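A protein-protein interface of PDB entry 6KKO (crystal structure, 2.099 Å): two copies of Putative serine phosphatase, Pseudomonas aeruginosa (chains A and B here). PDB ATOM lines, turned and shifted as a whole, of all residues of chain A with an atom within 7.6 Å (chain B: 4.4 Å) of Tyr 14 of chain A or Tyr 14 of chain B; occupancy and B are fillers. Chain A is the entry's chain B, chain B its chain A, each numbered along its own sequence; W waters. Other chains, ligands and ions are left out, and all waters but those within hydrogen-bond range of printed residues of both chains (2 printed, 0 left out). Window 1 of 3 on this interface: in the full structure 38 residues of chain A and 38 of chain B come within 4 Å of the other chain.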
ATOM      1  N   LEU A   7     -23.197 -24.819   4.419  1.00  0.00           N
ATOM      2  CA  LEU A   7     -23.443 -26.132   3.835  1.00  0.00           C
ATOM      3  C   LEU A   7     -24.703 -26.128   2.982  1.00  0.00           C
ATOM      4  O   LEU A   7     -24.766 -26.825   1.963  1.00  0.00           O
ATOM      5  CB  LEU A   7     -23.555 -27.186   4.934  1.00  0.00           C
ATOM      6  CG  LEU A   7     -23.447 -28.642   4.482  1.00  0.00           C
ATOM      7  CD1 LEU A   7     -22.075 -28.926   3.891  1.00  0.00           C
ATOM      8  CD2 LEU A   7     -23.747 -29.579   5.636  1.00  0.00           C
ATOM      9  N   LEU A   8     -25.713 -25.350   3.379  1.00  0.00           N
ATOM     10  CA  LEU A   8     -26.914 -25.236   2.560  1.00  0.00           C
ATOM     11  C   LEU A   8     -26.645 -24.406   1.312  1.00  0.00           C
ATOM     12  O   LEU A   8     -27.131 -24.736   0.225  1.00  0.00           O
ATOM     13  CB  LEU A   8     -28.056 -24.633   3.375  1.00  0.00           C
ATOM     14  CG  LEU A   8     -29.333 -24.356   2.578  1.00  0.00           C
ATOM     15  CD1 LEU A   8     -29.909 -25.648   2.006  1.00  0.00           C
ATOM     16  CD2 LEU A   8     -30.359 -23.614   3.427  1.00  0.00           C
ATOM     17  N   ALA A   9     -25.856 -23.336   1.446  1.00  0.00           N
ATOM     18  CA  ALA A   9     -25.524 -22.509   0.290  1.00  0.00           C
ATOM     19  C   ALA A   9     -24.729 -23.299  -0.742  1.00  0.00           C
ATOM     20  O   ALA A   9     -24.898 -23.104  -1.952  1.00  0.00           O
ATOM     21  CB  ALA A   9     -24.744 -21.270   0.733  1.00  0.00           C
ATOM     22  N   MET A  10     -23.864 -24.198  -0.284  1.00  0.00           N
ATOM     23  CA  MET A  10     -23.109 -25.069  -1.175  1.00  0.00           C
ATOM     24  C   MET A  10     -24.027 -26.044  -1.903  1.00  0.00           C
ATOM     25  O   MET A  10     -23.959 -26.173  -3.126  1.00  0.00           O
ATOM     26  CB  MET A  10     -22.047 -25.843  -0.394  1.00  0.00           C
ATOM     27  CG  MET A  10     -20.729 -25.113  -0.208  1.00  0.00           C
ATOM     28  SD  MET A  10     -19.605 -26.047   1.086  1.00  0.00           S
ATOM     29  CE  MET A  10     -20.185 -27.867   0.692  1.00  0.00           C
ATOM     30  N   ARG A  11     -24.879 -26.733  -1.138  1.00  0.00           N
ATOM     31  CA  ARG A  11     -25.801 -27.696  -1.732  1.00  0.00           C
ATOM     32  C   ARG A  11     -26.689 -27.042  -2.783  1.00  0.00           C
ATOM     33  O   ARG A  11     -26.976 -27.642  -3.825  1.00  0.00           O
ATOM     34  CB  ARG A  11     -26.650 -28.352  -0.644  1.00  0.00           C
ATOM     35  CG  ARG A  11     -27.626 -29.402  -1.156  1.00  0.00           C
ATOM     36  CD  ARG A  11     -26.933 -30.476  -1.978  1.00  0.00           C
ATOM     37  NE  ARG A  11     -27.883 -31.486  -2.438  1.00  0.00           N
ATOM     38  CZ  ARG A  11     -28.001 -32.699  -1.910  1.00  0.00           C
ATOM     39  NH1 ARG A  11     -27.222 -33.065  -0.900  1.00  0.00           N
ATOM     40  NH2 ARG A  11     -28.897 -33.550  -2.393  1.00  0.00           N
ATOM     41  N   GLU A  12     -27.126 -25.804  -2.534  1.00  0.00           N
ATOM     42  CA  GLU A  12     -27.968 -25.121  -3.510  1.00  0.00           C
ATOM     43  C   GLU A  12     -27.171 -24.718  -4.741  1.00  0.00           C
ATOM     44  O   GLU A  12     -27.687 -24.770  -5.864  1.00  0.00           O
ATOM     45  CB  GLU A  12     -28.637 -23.903  -2.874  1.00  0.00           C
ATOM     46  CG  GLU A  12     -29.571 -24.238  -1.725  1.00  0.00           C
ATOM     47  CD  GLU A  12     -30.189 -23.004  -1.099  1.00  0.00           C
ATOM     48  OE1 GLU A  12     -31.331 -23.098  -0.603  1.00  0.00           O
ATOM     49  OE2 GLU A  12     -29.538 -21.938  -1.115  1.00  0.00           O
ATOM     50  N   SER A  13     -25.913 -24.314  -4.552  1.00  0.00           N
ATOM     51  CA  SER A  13     -25.062 -23.997  -5.694  1.00  0.00           C
ATOM     52  C   SER A  13     -24.814 -25.230  -6.556  1.00  0.00           C
ATOM     53  O   SER A  13     -24.790 -25.138  -7.789  1.00  0.00           O
ATOM     54  CB  SER A  13     -23.740 -23.398  -5.216  1.00  0.00           C
ATOM     55  OG  SER A  13     -22.870 -23.151  -6.307  1.00  0.00           O
ATOM     56  N   TYR A  14     -24.631 -26.397  -5.929  1.00  0.00           N
ATOM     57  CA  TYR A  14     -24.462 -27.625  -6.701  1.00  0.00           C
ATOM     58  C   TYR A  14     -25.718 -27.943  -7.508  1.00  0.00           C
ATOM     59  O   TYR A  14     -25.631 -28.433  -8.640  1.00  0.00           O
ATOM     60  CB  TYR A  14     -24.098 -28.792  -5.782  1.00  0.00           C
ATOM     61  CG  TYR A  14     -22.813 -28.592  -5.008  1.00  0.00           C
ATOM     62  CD1 TYR A  14     -21.800 -27.777  -5.501  1.00  0.00           C
ATOM     63  CD2 TYR A  14     -22.605 -29.231  -3.792  1.00  0.00           C
ATOM     64  CE1 TYR A  14     -20.623 -27.590  -4.795  1.00  0.00           C
ATOM     65  CE2 TYR A  14     -21.428 -29.056  -3.082  1.00  0.00           C
ATOM     66  CZ  TYR A  14     -20.441 -28.235  -3.589  1.00  0.00           C
ATOM     67  OH  TYR A  14     -19.267 -28.055  -2.887  1.00  0.00           O
ATOM     68  N   THR A  15     -26.898 -27.675  -6.937  1.00  0.00           N
ATOM     69  CA  THR A  15     -28.148 -27.892  -7.665  1.00  0.00           C
ATOM     70  C   THR A  15     -28.233 -26.990  -8.889  1.00  0.00           C
ATOM     71  O   THR A  15     -28.587 -27.443  -9.984  1.00  0.00           O
ATOM     72  CB  THR A  15     -29.350 -27.646  -6.750  1.00  0.00           C
ATOM     73  OG1 THR A  15     -29.337 -28.588  -5.670  1.00  0.00           O
ATOM     74  CG2 THR A  15     -30.651 -27.792  -7.533  1.00  0.00           C
ATOM     75  N   ARG A  16     -27.915 -25.704  -8.722  1.00  0.00           N
ATOM     76  CA  ARG A  16     -27.999 -24.776  -9.844  1.00  0.00           C
ATOM     77  C   ARG A  16     -27.028 -25.150 -10.955  1.00  0.00           C
ATOM     78  O   ARG A  16     -27.265 -24.821 -12.124  1.00  0.00           O
ATOM     79  CB  ARG A  16     -27.736 -23.347  -9.369  1.00  0.00           C
ATOM     80  CG  ARG A  16     -28.787 -22.801  -8.416  1.00  0.00           C
ATOM     81  CD  ARG A  16     -28.576 -21.315  -8.157  1.00  0.00           C
ATOM     82  NE  ARG A  16     -27.309 -21.048  -7.481  1.00  0.00           N
ATOM     83  CZ  ARG A  16     -27.174 -20.941  -6.164  1.00  0.00           C
ATOM     84  NH1 ARG A  16     -28.232 -21.075  -5.373  1.00  0.00           N
ATOM     85  NH2 ARG A  16     -25.982 -20.696  -5.635  1.00  0.00           N
ATOM     86  N   GLN A  17     -25.939 -25.833 -10.619  1.00  0.00           N
ATOM     87  CA  GLN A  17     -24.965 -26.260 -11.615  1.00  0.00           C
ATOM     88  C   GLN A  17     -25.229 -27.658 -12.147  1.00  0.00           C
ATOM     89  O   GLN A  17     -24.470 -28.129 -13.000  1.00  0.00           O
ATOM     90  CB  GLN A  17     -23.544 -26.189 -11.024  1.00  0.00           C
ATOM     91  CG  GLN A  17     -23.231 -24.822 -10.393  1.00  0.00           C
ATOM     92  CD  GLN A  17     -21.853 -24.717  -9.776  1.00  0.00           C
ATOM     93  OE1 GLN A  17     -20.841 -24.849 -10.470  1.00  0.00           O
ATOM     94  NE2 GLN A  17     -21.803 -24.442  -8.472  1.00  0.00           N
ATOM     95  N   ARG A  18     -26.285 -28.323 -11.663  1.00  0.00           N
ATOM     96  CA  ARG A  18     -26.613 -29.691 -12.061  1.00  0.00           C
ATOM     97  C   ARG A  18     -25.427 -30.622 -11.818  1.00  0.00           C
ATOM     98  O   ARG A  18     -25.132 -31.507 -12.625  1.00  0.00           O
ATOM     99  CB  ARG A  18     -27.089 -29.765 -13.517  1.00  0.00           C
ATOM    100  CG  ARG A  18     -28.327 -28.922 -13.822  1.00  0.00           C
ATOM    101  CD  ARG A  18     -28.583 -28.847 -15.322  1.00  0.00           C
ATOM    102  NE  ARG A  18     -29.798 -28.107 -15.650  1.00  0.00           N
ATOM    103  CZ  ARG A  18     -30.980 -28.674 -15.866  1.00  0.00           C
ATOM    104  NH1 ARG A  18     -31.106 -29.992 -15.786  1.00  0.00           N
ATOM    105  NH2 ARG A  18     -32.036 -27.927 -16.161  1.00  0.00           N
ATOM    106  N   ILE A  19     -24.744 -30.418 -10.693  1.00  0.00           N
ATOM    107  CA  ILE A  19     -23.586 -31.228 -10.334  1.00  0.00           C
ATOM    108  C   ILE A  19     -24.074 -32.549  -9.762  1.00  0.00           C
ATOM    109  O   ILE A  19     -24.894 -32.574  -8.836  1.00  0.00           O
ATOM    110  CB  ILE A  19     -22.687 -30.492  -9.326  1.00  0.00           C
ATOM    111  CG1 ILE A  19     -22.072 -29.241  -9.951  1.00  0.00           C
ATOM    112  CG2 ILE A  19     -21.598 -31.424  -8.813  1.00  0.00           C
ATOM    113  CD1 ILE A  19     -21.177 -28.471  -8.994  1.00  0.00           C
ATOM    114  N   LEU A  20     -23.573 -33.650 -10.315  1.00  0.00           N
ATOM    115  CA  LEU A  20     -23.921 -34.970  -9.813  1.00  0.00           C
ATOM    116  C   LEU A  20     -22.965 -35.421  -8.712  1.00  0.00           C
ATOM    117  O   LEU A  20     -23.395 -35.971  -7.692  1.00  0.00           O
ATOM    118  CB  LEU A  20     -23.892 -35.979 -10.965  1.00  0.00           C
ATOM    119  CG  LEU A  20     -24.396 -35.462 -12.310  1.00  0.00           C
ATOM    120  CD1 LEU A  20     -24.166 -36.477 -13.464  1.00  0.00           C
ATOM    121  CD2 LEU A  20     -25.862 -34.925 -12.209  1.00  0.00           C
ATOM    122  N   LEU A  21     -21.666 -35.202  -8.926  1.00  0.00           N
ATOM    123  CA  LEU A  21     -20.608 -35.524  -7.980  1.00  0.00           C
ATOM    124  C   LEU A  21     -19.585 -34.402  -7.998  1.00  0.00           C
ATOM    125  O   LEU A  21     -19.322 -33.798  -9.044  1.00  0.00           O
ATOM    126  CB  LEU A  21     -19.895 -36.843  -8.329  1.00  0.00           C
ATOM    127  CG  LEU A  21     -20.483 -38.210  -8.007  1.00  0.00           C
ATOM    128  CD1 LEU A  21     -20.061 -39.208  -9.070  1.00  0.00           C
ATOM    129  CD2 LEU A  21     -19.993 -38.660  -6.652  1.00  0.00           C
ATOM    130  N   CYS A  22     -18.989 -34.144  -6.841  1.00  0.00           N
ATOM    131  CA  CYS A  22     -17.865 -33.222  -6.774  1.00  0.00           C
ATOM    132  C   CYS A  22     -17.072 -33.519  -5.513  1.00  0.00           C
ATOM    133  O   CYS A  22     -17.642 -33.860  -4.473  1.00  0.00           O
ATOM    134  CB  CYS A  22     -18.316 -31.759  -6.802  1.00  0.00           C
ATOM    135  SG  CYS A  22     -19.378 -31.312  -5.449  1.00  0.00           S
ATOM    136  N   PHE A  23     -15.754 -33.415  -5.635  1.00  0.00           N
ATOM    137  CA  PHE A  23     -14.830 -33.681  -4.552  1.00  0.00           C
ATOM    138  C   PHE A  23     -13.741 -32.626  -4.571  1.00  0.00           C
ATOM    139  O   PHE A  23     -13.341 -32.143  -5.634  1.00  0.00           O
ATOM    140  CB  PHE A  23     -14.200 -35.074  -4.657  1.00  0.00           C
ATOM    141  CG  PHE A  23     -13.086 -35.296  -3.687  1.00  0.00           C
ATOM    142  CD1 PHE A  23     -13.350 -35.644  -2.371  1.00  0.00           C
ATOM    143  CD2 PHE A  23     -11.761 -35.141  -4.084  1.00  0.00           C
ATOM    144  CE1 PHE A  23     -12.318 -35.842  -1.473  1.00  0.00           C
ATOM    145  CE2 PHE A  23     -10.727 -35.334  -3.190  1.00  0.00           C
ATOM    146  CZ  PHE A  23     -11.007 -35.682  -1.884  1.00  0.00           C
ATOM    147  N   ASN A  24     -13.286 -32.257  -3.379  1.00  0.00           N
ATOM    148  CA  ASN A  24     -12.196 -31.313  -3.207  1.00  0.00           C
ATOM    149  C   ASN A  24     -11.348 -31.784  -2.040  1.00  0.00           C
ATOM    150  O   ASN A  24     -11.874 -32.025  -0.949  1.00  0.00           O
ATOM    151  CB  ASN A  24     -12.717 -29.892  -2.957  1.00  0.00           C
ATOM    152  CG  ASN A  24     -11.603 -28.904  -2.640  1.00  0.00           C
ATOM    153  OD1 ASN A  24     -11.054 -28.271  -3.538  1.00  0.00           O
ATOM    154  ND2 ASN A  24     -11.282 -28.756  -1.360  1.00  0.00           N
ATOM    155  N   GLY A  25     -10.048 -31.919  -2.275  1.00  0.00           N
ATOM    156  CA  GLY A  25      -9.125 -32.327  -1.250  1.00  0.00           C
ATOM    157  C   GLY A  25      -8.037 -33.220  -1.802  1.00  0.00           C
ATOM    158  O   GLY A  25      -7.933 -33.438  -3.017  1.00  0.00           O
ATOM    159  N   ALA A  83      -6.743 -31.610  -5.266  1.00  0.00           N
ATOM    160  CA  ALA A  83      -7.487 -31.393  -6.502  1.00  0.00           C
ATOM    161  C   ALA A  83      -8.945 -31.065  -6.214  1.00  0.00           C
ATOM    162  O   ALA A  83      -9.471 -31.338  -5.130  1.00  0.00           O
ATOM    163  CB  ALA A  83      -7.404 -32.611  -7.428  1.00  0.00           C
ATOM    164  N   THR A  84      -9.592 -30.487  -7.225  1.00  0.00           N
ATOM    165  CA  THR A  84     -11.021 -30.202  -7.228  1.00  0.00           C
ATOM    166  C   THR A  84     -11.607 -30.838  -8.479  1.00  0.00           C
ATOM    167  O   THR A  84     -11.195 -30.500  -9.593  1.00  0.00           O
ATOM    168  CB  THR A  84     -11.294 -28.694  -7.222  1.00  0.00           C
ATOM    169  OG1 THR A  84     -10.665 -28.089  -6.086  1.00  0.00           O
ATOM    170  CG2 THR A  84     -12.796 -28.421  -7.170  1.00  0.00           C
ATOM    171  N   VAL A  85     -12.540 -31.774  -8.303  1.00  0.00           N
ATOM    172  CA  VAL A  85     -13.147 -32.490  -9.419  1.00  0.00           C
ATOM    173  C   VAL A  85     -14.660 -32.350  -9.332  1.00  0.00           C
ATOM    174  O   VAL A  85     -15.240 -32.470  -8.246  1.00  0.00           O
ATOM    175  CB  VAL A  85     -12.747 -33.978  -9.419  1.00  0.00           C
ATOM    176  CG1 VAL A  85     -13.122 -34.625 -10.744  1.00  0.00           C
ATOM    177  CG2 VAL A  85     -11.263 -34.131  -9.133  1.00  0.00           C
ATOM    178  N   ALA A  86     -15.306 -32.120 -10.474  1.00  0.00           N
ATOM    179  CA  ALA A  86     -16.759 -31.986 -10.523  1.00  0.00           C
ATOM    180  C   ALA A  86     -17.302 -32.635 -11.787  1.00  0.00           C
ATOM    181  O   ALA A  86     -16.691 -32.541 -12.855  1.00  0.00           O
ATOM    182  CB  ALA A  86     -17.195 -30.520 -10.477  1.00  0.00           C
ATOM    183  N   ILE A  87     -18.455 -33.289 -11.665  1.00  0.00           N
ATOM    184  CA  ILE A  87     -19.137 -33.883 -12.809  1.00  0.00           C
ATOM    185  C   ILE A  87     -20.588 -33.421 -12.788  1.00  0.00           C
ATOM    186  O   ILE A  87     -21.297 -33.632 -11.793  1.00  0.00           O
ATOM    187  CB  ILE A  87     -19.053 -35.413 -12.806  1.00  0.00           C
ATOM    188  CG1 ILE A  87     -17.588 -35.857 -12.801  1.00  0.00           C
ATOM    189  CG2 ILE A  87     -19.788 -35.967 -14.016  1.00  0.00           C
ATOM    190  CD1 ILE A  87     -17.399 -37.333 -12.649  1.00  0.00           C
ATOM    191  N   ALA A  88     -21.017 -32.770 -13.864  1.00  0.00           N
ATOM    192  CA  ALA A  88     -22.357 -32.217 -13.991  1.00  0.00           C
ATOM    193  C   ALA A  88     -23.040 -32.780 -15.232  1.00  0.00           C
ATOM    194  O   ALA A  88     -22.442 -33.509 -16.023  1.00  0.00           O
ATOM    195  CB  ALA A  88     -22.314 -30.684 -14.064  1.00  0.00           C
ATOM    196  N   MET B  10     -15.922 -22.443  -6.880  1.00  0.00           N
ATOM    197  CA  MET B  10     -16.015 -23.409  -5.789  1.00  0.00           C
ATOM    198  C   MET B  10     -14.716 -23.472  -5.004  1.00  0.00           C
ATOM    199  O   MET B  10     -14.729 -23.429  -3.774  1.00  0.00           O
ATOM    200  CB  MET B  10     -16.372 -24.805  -6.308  1.00  0.00           C
ATOM    201  CG  MET B  10     -17.792 -24.942  -6.824  1.00  0.00           C
ATOM    202  SD  MET B  10     -18.024 -26.524  -7.944  1.00  0.00           S
ATOM    203  CE  MET B  10     -17.156 -27.855  -6.808  1.00  0.00           C
ATOM    204  N   ARG B  11     -13.595 -23.564  -5.728  1.00  0.00           N
ATOM    205  CA  ARG B  11     -12.296 -23.644  -5.070  1.00  0.00           C
ATOM    206  C   ARG B  11     -12.073 -22.449  -4.149  1.00  0.00           C
ATOM    207  O   ARG B  11     -11.513 -22.592  -3.056  1.00  0.00           O
ATOM    208  CB  ARG B  11     -11.189 -23.741  -6.120  1.00  0.00           C
ATOM    209  CG  ARG B  11      -9.794 -23.920  -5.544  1.00  0.00           C
ATOM    210  CD  ARG B  11      -9.755 -25.122  -4.613  1.00  0.00           C
ATOM    211  NE  ARG B  11      -8.425 -25.362  -4.061  1.00  0.00           N
ATOM    212  CZ  ARG B  11      -7.614 -26.335  -4.465  1.00  0.00           C
ATOM    213  NH1 ARG B  11      -7.999 -27.167  -5.424  1.00  0.00           N
ATOM    214  NH2 ARG B  11      -6.419 -26.480  -3.906  1.00  0.00           N
ATOM    215  N   GLU B  12     -12.519 -21.263  -4.571  1.00  0.00           N
ATOM    216  CA  GLU B  12     -12.367 -20.068  -3.748  1.00  0.00           C
ATOM    217  C   GLU B  12     -13.323 -20.086  -2.560  1.00  0.00           C
ATOM    218  O   GLU B  12     -12.981 -19.609  -1.470  1.00  0.00           O
ATOM    219  CB  GLU B  12     -12.577 -18.828  -4.611  1.00  0.00           C
ATOM    220  CG  GLU B  12     -11.567 -18.747  -5.754  1.00  0.00           C
ATOM    221  CD  GLU B  12     -11.789 -17.546  -6.650  1.00  0.00           C
ATOM    222  OE1 GLU B  12     -10.807 -17.034  -7.220  1.00  0.00           O
ATOM    223  OE2 GLU B  12     -12.945 -17.110  -6.782  1.00  0.00           O
ATOM    224  N   SER B  13     -14.537 -20.615  -2.751  1.00  0.00           N
ATOM    225  CA  SER B  13     -15.464 -20.755  -1.631  1.00  0.00           C
ATOM    226  C   SER B  13     -14.913 -21.718  -0.586  1.00  0.00           C
ATOM    227  O   SER B  13     -15.071 -21.496   0.621  1.00  0.00           O
ATOM    228  CB  SER B  13     -16.826 -21.228  -2.137  1.00  0.00           C
ATOM    229  OG  SER B  13     -17.715 -21.450  -1.057  1.00  0.00           O
ATOM    230  N   TYR B  14     -14.263 -22.796  -1.033  1.00  0.00           N
ATOM    231  CA  TYR B  14     -13.629 -23.718  -0.099  1.00  0.00           C
ATOM    232  C   TYR B  14     -12.519 -23.028   0.680  1.00  0.00           C
ATOM    233  O   TYR B  14     -12.373 -23.241   1.890  1.00  0.00           O
ATOM    234  CB  TYR B  14     -13.078 -24.922  -0.863  1.00  0.00           C
ATOM    235  CG  TYR B  14     -14.123 -25.722  -1.601  1.00  0.00           C
ATOM    236  CD1 TYR B  14     -15.430 -25.791  -1.136  1.00  0.00           C
ATOM    237  CD2 TYR B  14     -13.810 -26.393  -2.778  1.00  0.00           C
ATOM    238  CE1 TYR B  14     -16.392 -26.522  -1.804  1.00  0.00           C
ATOM    239  CE2 TYR B  14     -14.770 -27.125  -3.460  1.00  0.00           C
ATOM    240  CZ  TYR B  14     -16.058 -27.184  -2.967  1.00  0.00           C
ATOM    241  OH  TYR B  14     -17.024 -27.911  -3.630  1.00  0.00           O
ATOM    242  N   THR B  15     -11.734 -22.182   0.002  1.00  0.00           N
ATOM    243  CA  THR B  15     -10.685 -21.424   0.679  1.00  0.00           C
ATOM    244  C   THR B  15     -11.273 -20.457   1.698  1.00  0.00           C
ATOM    245  O   THR B  15     -10.746 -20.319   2.808  1.00  0.00           O
ATOM    246  CB  THR B  15      -9.831 -20.670  -0.345  1.00  0.00           C
ATOM    247  OG1 THR B  15      -9.170 -21.604  -1.207  1.00  0.00           O
ATOM    248  CG2 THR B  15      -8.784 -19.811   0.353  1.00  0.00           C
ATOM    249  N   ARG B  16     -12.368 -19.779   1.340  1.00  0.00           N
ATOM    250  CA  ARG B  16     -13.002 -18.846   2.270  1.00  0.00           C
ATOM    251  C   ARG B  16     -13.430 -19.543   3.556  1.00  0.00           C
ATOM    252  O   ARG B  16     -13.237 -19.008   4.655  1.00  0.00           O
ATOM    253  CB  ARG B  16     -14.203 -18.174   1.605  1.00  0.00           C
ATOM    254  CG  ARG B  16     -14.894 -17.144   2.487  1.00  0.00           C
ATOM    255  CD  ARG B  16     -16.180 -16.613   1.863  1.00  0.00           C
ATOM    256  NE  ARG B  16     -17.239 -17.619   1.819  1.00  0.00           N
ATOM    257  CZ  ARG B  16     -17.658 -18.223   0.711  1.00  0.00           C
ATOM    258  NH1 ARG B  16     -18.629 -19.125   0.774  1.00  0.00           N
ATOM    259  NH2 ARG B  16     -17.115 -17.921  -0.462  1.00  0.00           N
ATOM    260  N   GLN B  17     -14.009 -20.735   3.441  1.00  0.00           N
ATOM    261  CA  GLN B  17     -14.501 -21.492   4.587  1.00  0.00           C
ATOM    262  C   GLN B  17     -13.429 -22.351   5.244  1.00  0.00           C
ATOM    263  O   GLN B  17     -13.737 -23.068   6.201  1.00  0.00           O
ATOM    264  CB  GLN B  17     -15.673 -22.386   4.165  1.00  0.00           C
ATOM    265  CG  GLN B  17     -16.789 -21.655   3.448  1.00  0.00           C
ATOM    266  CD  GLN B  17     -17.881 -22.593   2.970  1.00  0.00           C
ATOM    267  OE1 GLN B  17     -18.191 -22.643   1.779  1.00  0.00           O
ATOM    268  NE2 GLN B  17     -18.469 -23.342   3.896  1.00  0.00           N
ATOM    269  N   ARG B  18     -12.190 -22.305   4.745  1.00  0.00           N
ATOM    270  CA  ARG B  18     -11.082 -23.098   5.277  1.00  0.00           C
ATOM    271  C   ARG B  18     -11.393 -24.597   5.242  1.00  0.00           C
ATOM    272  O   ARG B  18     -11.053 -25.345   6.163  1.00  0.00           O
ATOM    273  CB  ARG B  18     -10.725 -22.650   6.695  1.00  0.00           C
ATOM    274  CG  ARG B  18     -10.350 -21.174   6.800  1.00  0.00           C
ATOM    275  CD  ARG B  18     -10.265 -20.717   8.252  1.00  0.00           C
ATOM    276  NE  ARG B  18      -9.144 -21.336   8.952  1.00  0.00           N
ATOM    277  CZ  ARG B  18      -7.931 -20.800   9.040  1.00  0.00           C
ATOM    278  NH1 ARG B  18      -7.678 -19.627   8.474  1.00  0.00           N
ATOM    279  NH2 ARG B  18      -6.970 -21.436   9.694  1.00  0.00           N
ATOM    280  N   ILE B  19     -12.040 -25.042   4.168  1.00  0.00           N
ATOM    281  CA  ILE B  19     -12.392 -26.450   4.006  1.00  0.00           C
ATOM    282  C   ILE B  19     -11.192 -27.221   3.471  1.00  0.00           C
ATOM    283  O   ILE B  19     -10.620 -26.861   2.436  1.00  0.00           O
ATOM    284  CB  ILE B  19     -13.603 -26.607   3.073  1.00  0.00           C
ATOM    285  CG1 ILE B  19     -14.847 -25.985   3.699  1.00  0.00           C
ATOM    286  CG2 ILE B  19     -13.840 -28.078   2.755  1.00  0.00           C
ATOM    287  CD1 ILE B  19     -16.068 -26.108   2.830  1.00  0.00           C
ATOM    288  N   CYS B  22     -14.134 -31.990   1.128  1.00  0.00           N
ATOM    289  CA  CYS B  22     -15.573 -31.913   0.953  1.00  0.00           C
ATOM    290  C   CYS B  22     -15.977 -32.811  -0.207  1.00  0.00           C
ATOM    291  O   CYS B  22     -15.249 -32.941  -1.196  1.00  0.00           O
ATOM    292  CB  CYS B  22     -16.029 -30.472   0.711  1.00  0.00           C
ATOM    293  SG  CYS B  22     -15.401 -29.773  -0.795  1.00  0.00           S
ATOM    294  N   ASN B  24     -19.713 -34.260  -2.354  1.00  0.00           N
ATOM    295  CA  ASN B  24     -21.145 -34.138  -2.600  1.00  0.00           C
ATOM    296  C   ASN B  24     -21.547 -35.172  -3.638  1.00  0.00           C
ATOM    297  O   ASN B  24     -20.959 -35.225  -4.722  1.00  0.00           O
ATOM    298  CB  ASN B  24     -21.515 -32.732  -3.100  1.00  0.00           C
ATOM    299  CG  ASN B  24     -22.977 -32.623  -3.516  1.00  0.00           C
ATOM    300  OD1 ASN B  24     -23.837 -32.277  -2.707  1.00  0.00           O
ATOM    301  ND2 ASN B  24     -23.262 -32.924  -4.779  1.00  0.00           N
HETATM  302  O   HOH W   1     -25.762 -33.277  -6.161  1.00  0.00           O
HETATM  303  O   HOH W   2      -9.109 -27.321   0.050  1.00  0.00           O
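NH1 of Arg 11 of chain B is in hydrogen-bond range of OG1 of Thr 84 of chain A (2.9 Å). OE1 of Gln 17 of chain B sits close to SD of Met 10 of chain A (3.8 Å). O of Cys 22 of chain B is in hydrogen-bond range of N of Asn 24 of chain A (3.0 Å). O of Cys 22 of chain A lies within hydrogen-bond range of N of Asn 24 of chain B. The side-chain hydroxyl of Tyr 14 of chain B lies close to the side-chain hydroxyl of Tyr 14 of chain A.
OG of Ser 13 of chain B lies within hydrogen-bond range of OE1 of Gln 17 of chain B, at 3.1 Å. OH of Tyr 14 of chain B sits close to SG of Cys 22 of chain B (3.8 Å). N of Leu 20 of chain A is in hydrogen-bond range of O of Ile 87 of chain A (2.7 Å). O of Leu 21 of chain A is in hydrogen-bond range of N of Ile 87 of chain A, at 2.8 Å. N of Val 85 of chain A lies within hydrogen-bond range of O of Phe 23 of chain A, at 2.8 Å. The side-chain amide oxygen (OD1) of Asn 24 of chain A sits at hydrogen-bond distance from the side-chain hydroxyl (OG1) of Thr 84 of chain A, at 2.6 Å.
Ile 19 of chain B touches Met 10 of chain A (CD1 to SD, 3.9 Å). Arg 11 of chain A touches Asn 24 of chain B. CD2 of Tyr 14 of chain A touches CG of Asn 24 of chain B (3.4 Å). CD1 of Ile 19 of chain A touches SD of Met 10 of chain B (3.9 Å). O of Leu 20 of chain A touches O of Asn 24 of chain B (3.9 Å). Leu 21 of chain A touches Asn 24 of chain B (CA to O, 3.3 Å). O of Cys 22 of chain B touches CA of Phe 23 of chain A, at 3.5 Å. Arg 11 of chain B touches Asn 24 of chain A (CD to OD1, 3.6 Å). Tyr 14 of chain B touches Asn 24 of chain A.
Of the printed residues of chain B, Tyr 14 of chain A touches Tyr 14 and Asn 24. Of chain A, only Tyr 14 and Asn 24 come within 4 Å of Tyr 14 of chain B. Printed residues of chain B within 4 Å of Leu 21 of chain A: Asn 24 (3.3 Å). Of the printed residues of chain B, Leu 20 of chain A touches Asn 24 (3.9 Å). Printed residues of chain A within 4 Å of Ile 19 of chain B: Met 10 (3.9 Å). Of the printed residues of chain A, Arg 11 of chain B touches Asn 24 and Thr 84. Of the printed residues of chain B, Thr 84 of chain A touches Arg 11 (2.9 Å). Val 85 of chain A touches none of the printed residues of chain B. Arg 16 of chain B touches none of the printed residues of chain A. The nearest residue of chain A that does not touch Tyr 14 of chain B is Met 10 of chain A (4.3 Å). The nearest printed residue of chain B that does not touch Leu 21 of chain A is Met 10 of chain B (6.7 Å).
Among the printed residues, no Asp or Glu carboxylate lies within 4 Å of a Lys or Arg side-chain nitrogen of the other chain.
Met 10 of chain A touches Gln 17 of chain B, but with the chains exchanged Gln 17 of chain A does not touch Met 10 of chain B (4.1 Å). Met 10 of chain A touches Ile 19 of chain B, and with the chains exchanged Ile 19 of chain A touches Met 10 of chain B. Arg 11 of chain A touches Asn 24 of chain B, and with the chains exchanged Asn 24 of chain A touches Arg 11 of chain B. Cys 22 of chain A touches Asn 24 of chain B, and with the chains exchanged Asn 24 of chain A touches Cys 22 of chain B. Positions printed for both chains: 10, 11, 12, 13, 14, 15, 16, 17, 18, 19, 22 and 24.
Water W2 bridges O of Ile 19 of chain B (2.9 Å) and ND2 of Asn 24 of chain A (3.0 Å). Water W1 bridges the side-chain amide nitrogen of Asn 24 of chain B (2.9 Å) and the backbone carbonyl oxygen of Ile 19 of chain A (2.9 Å).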
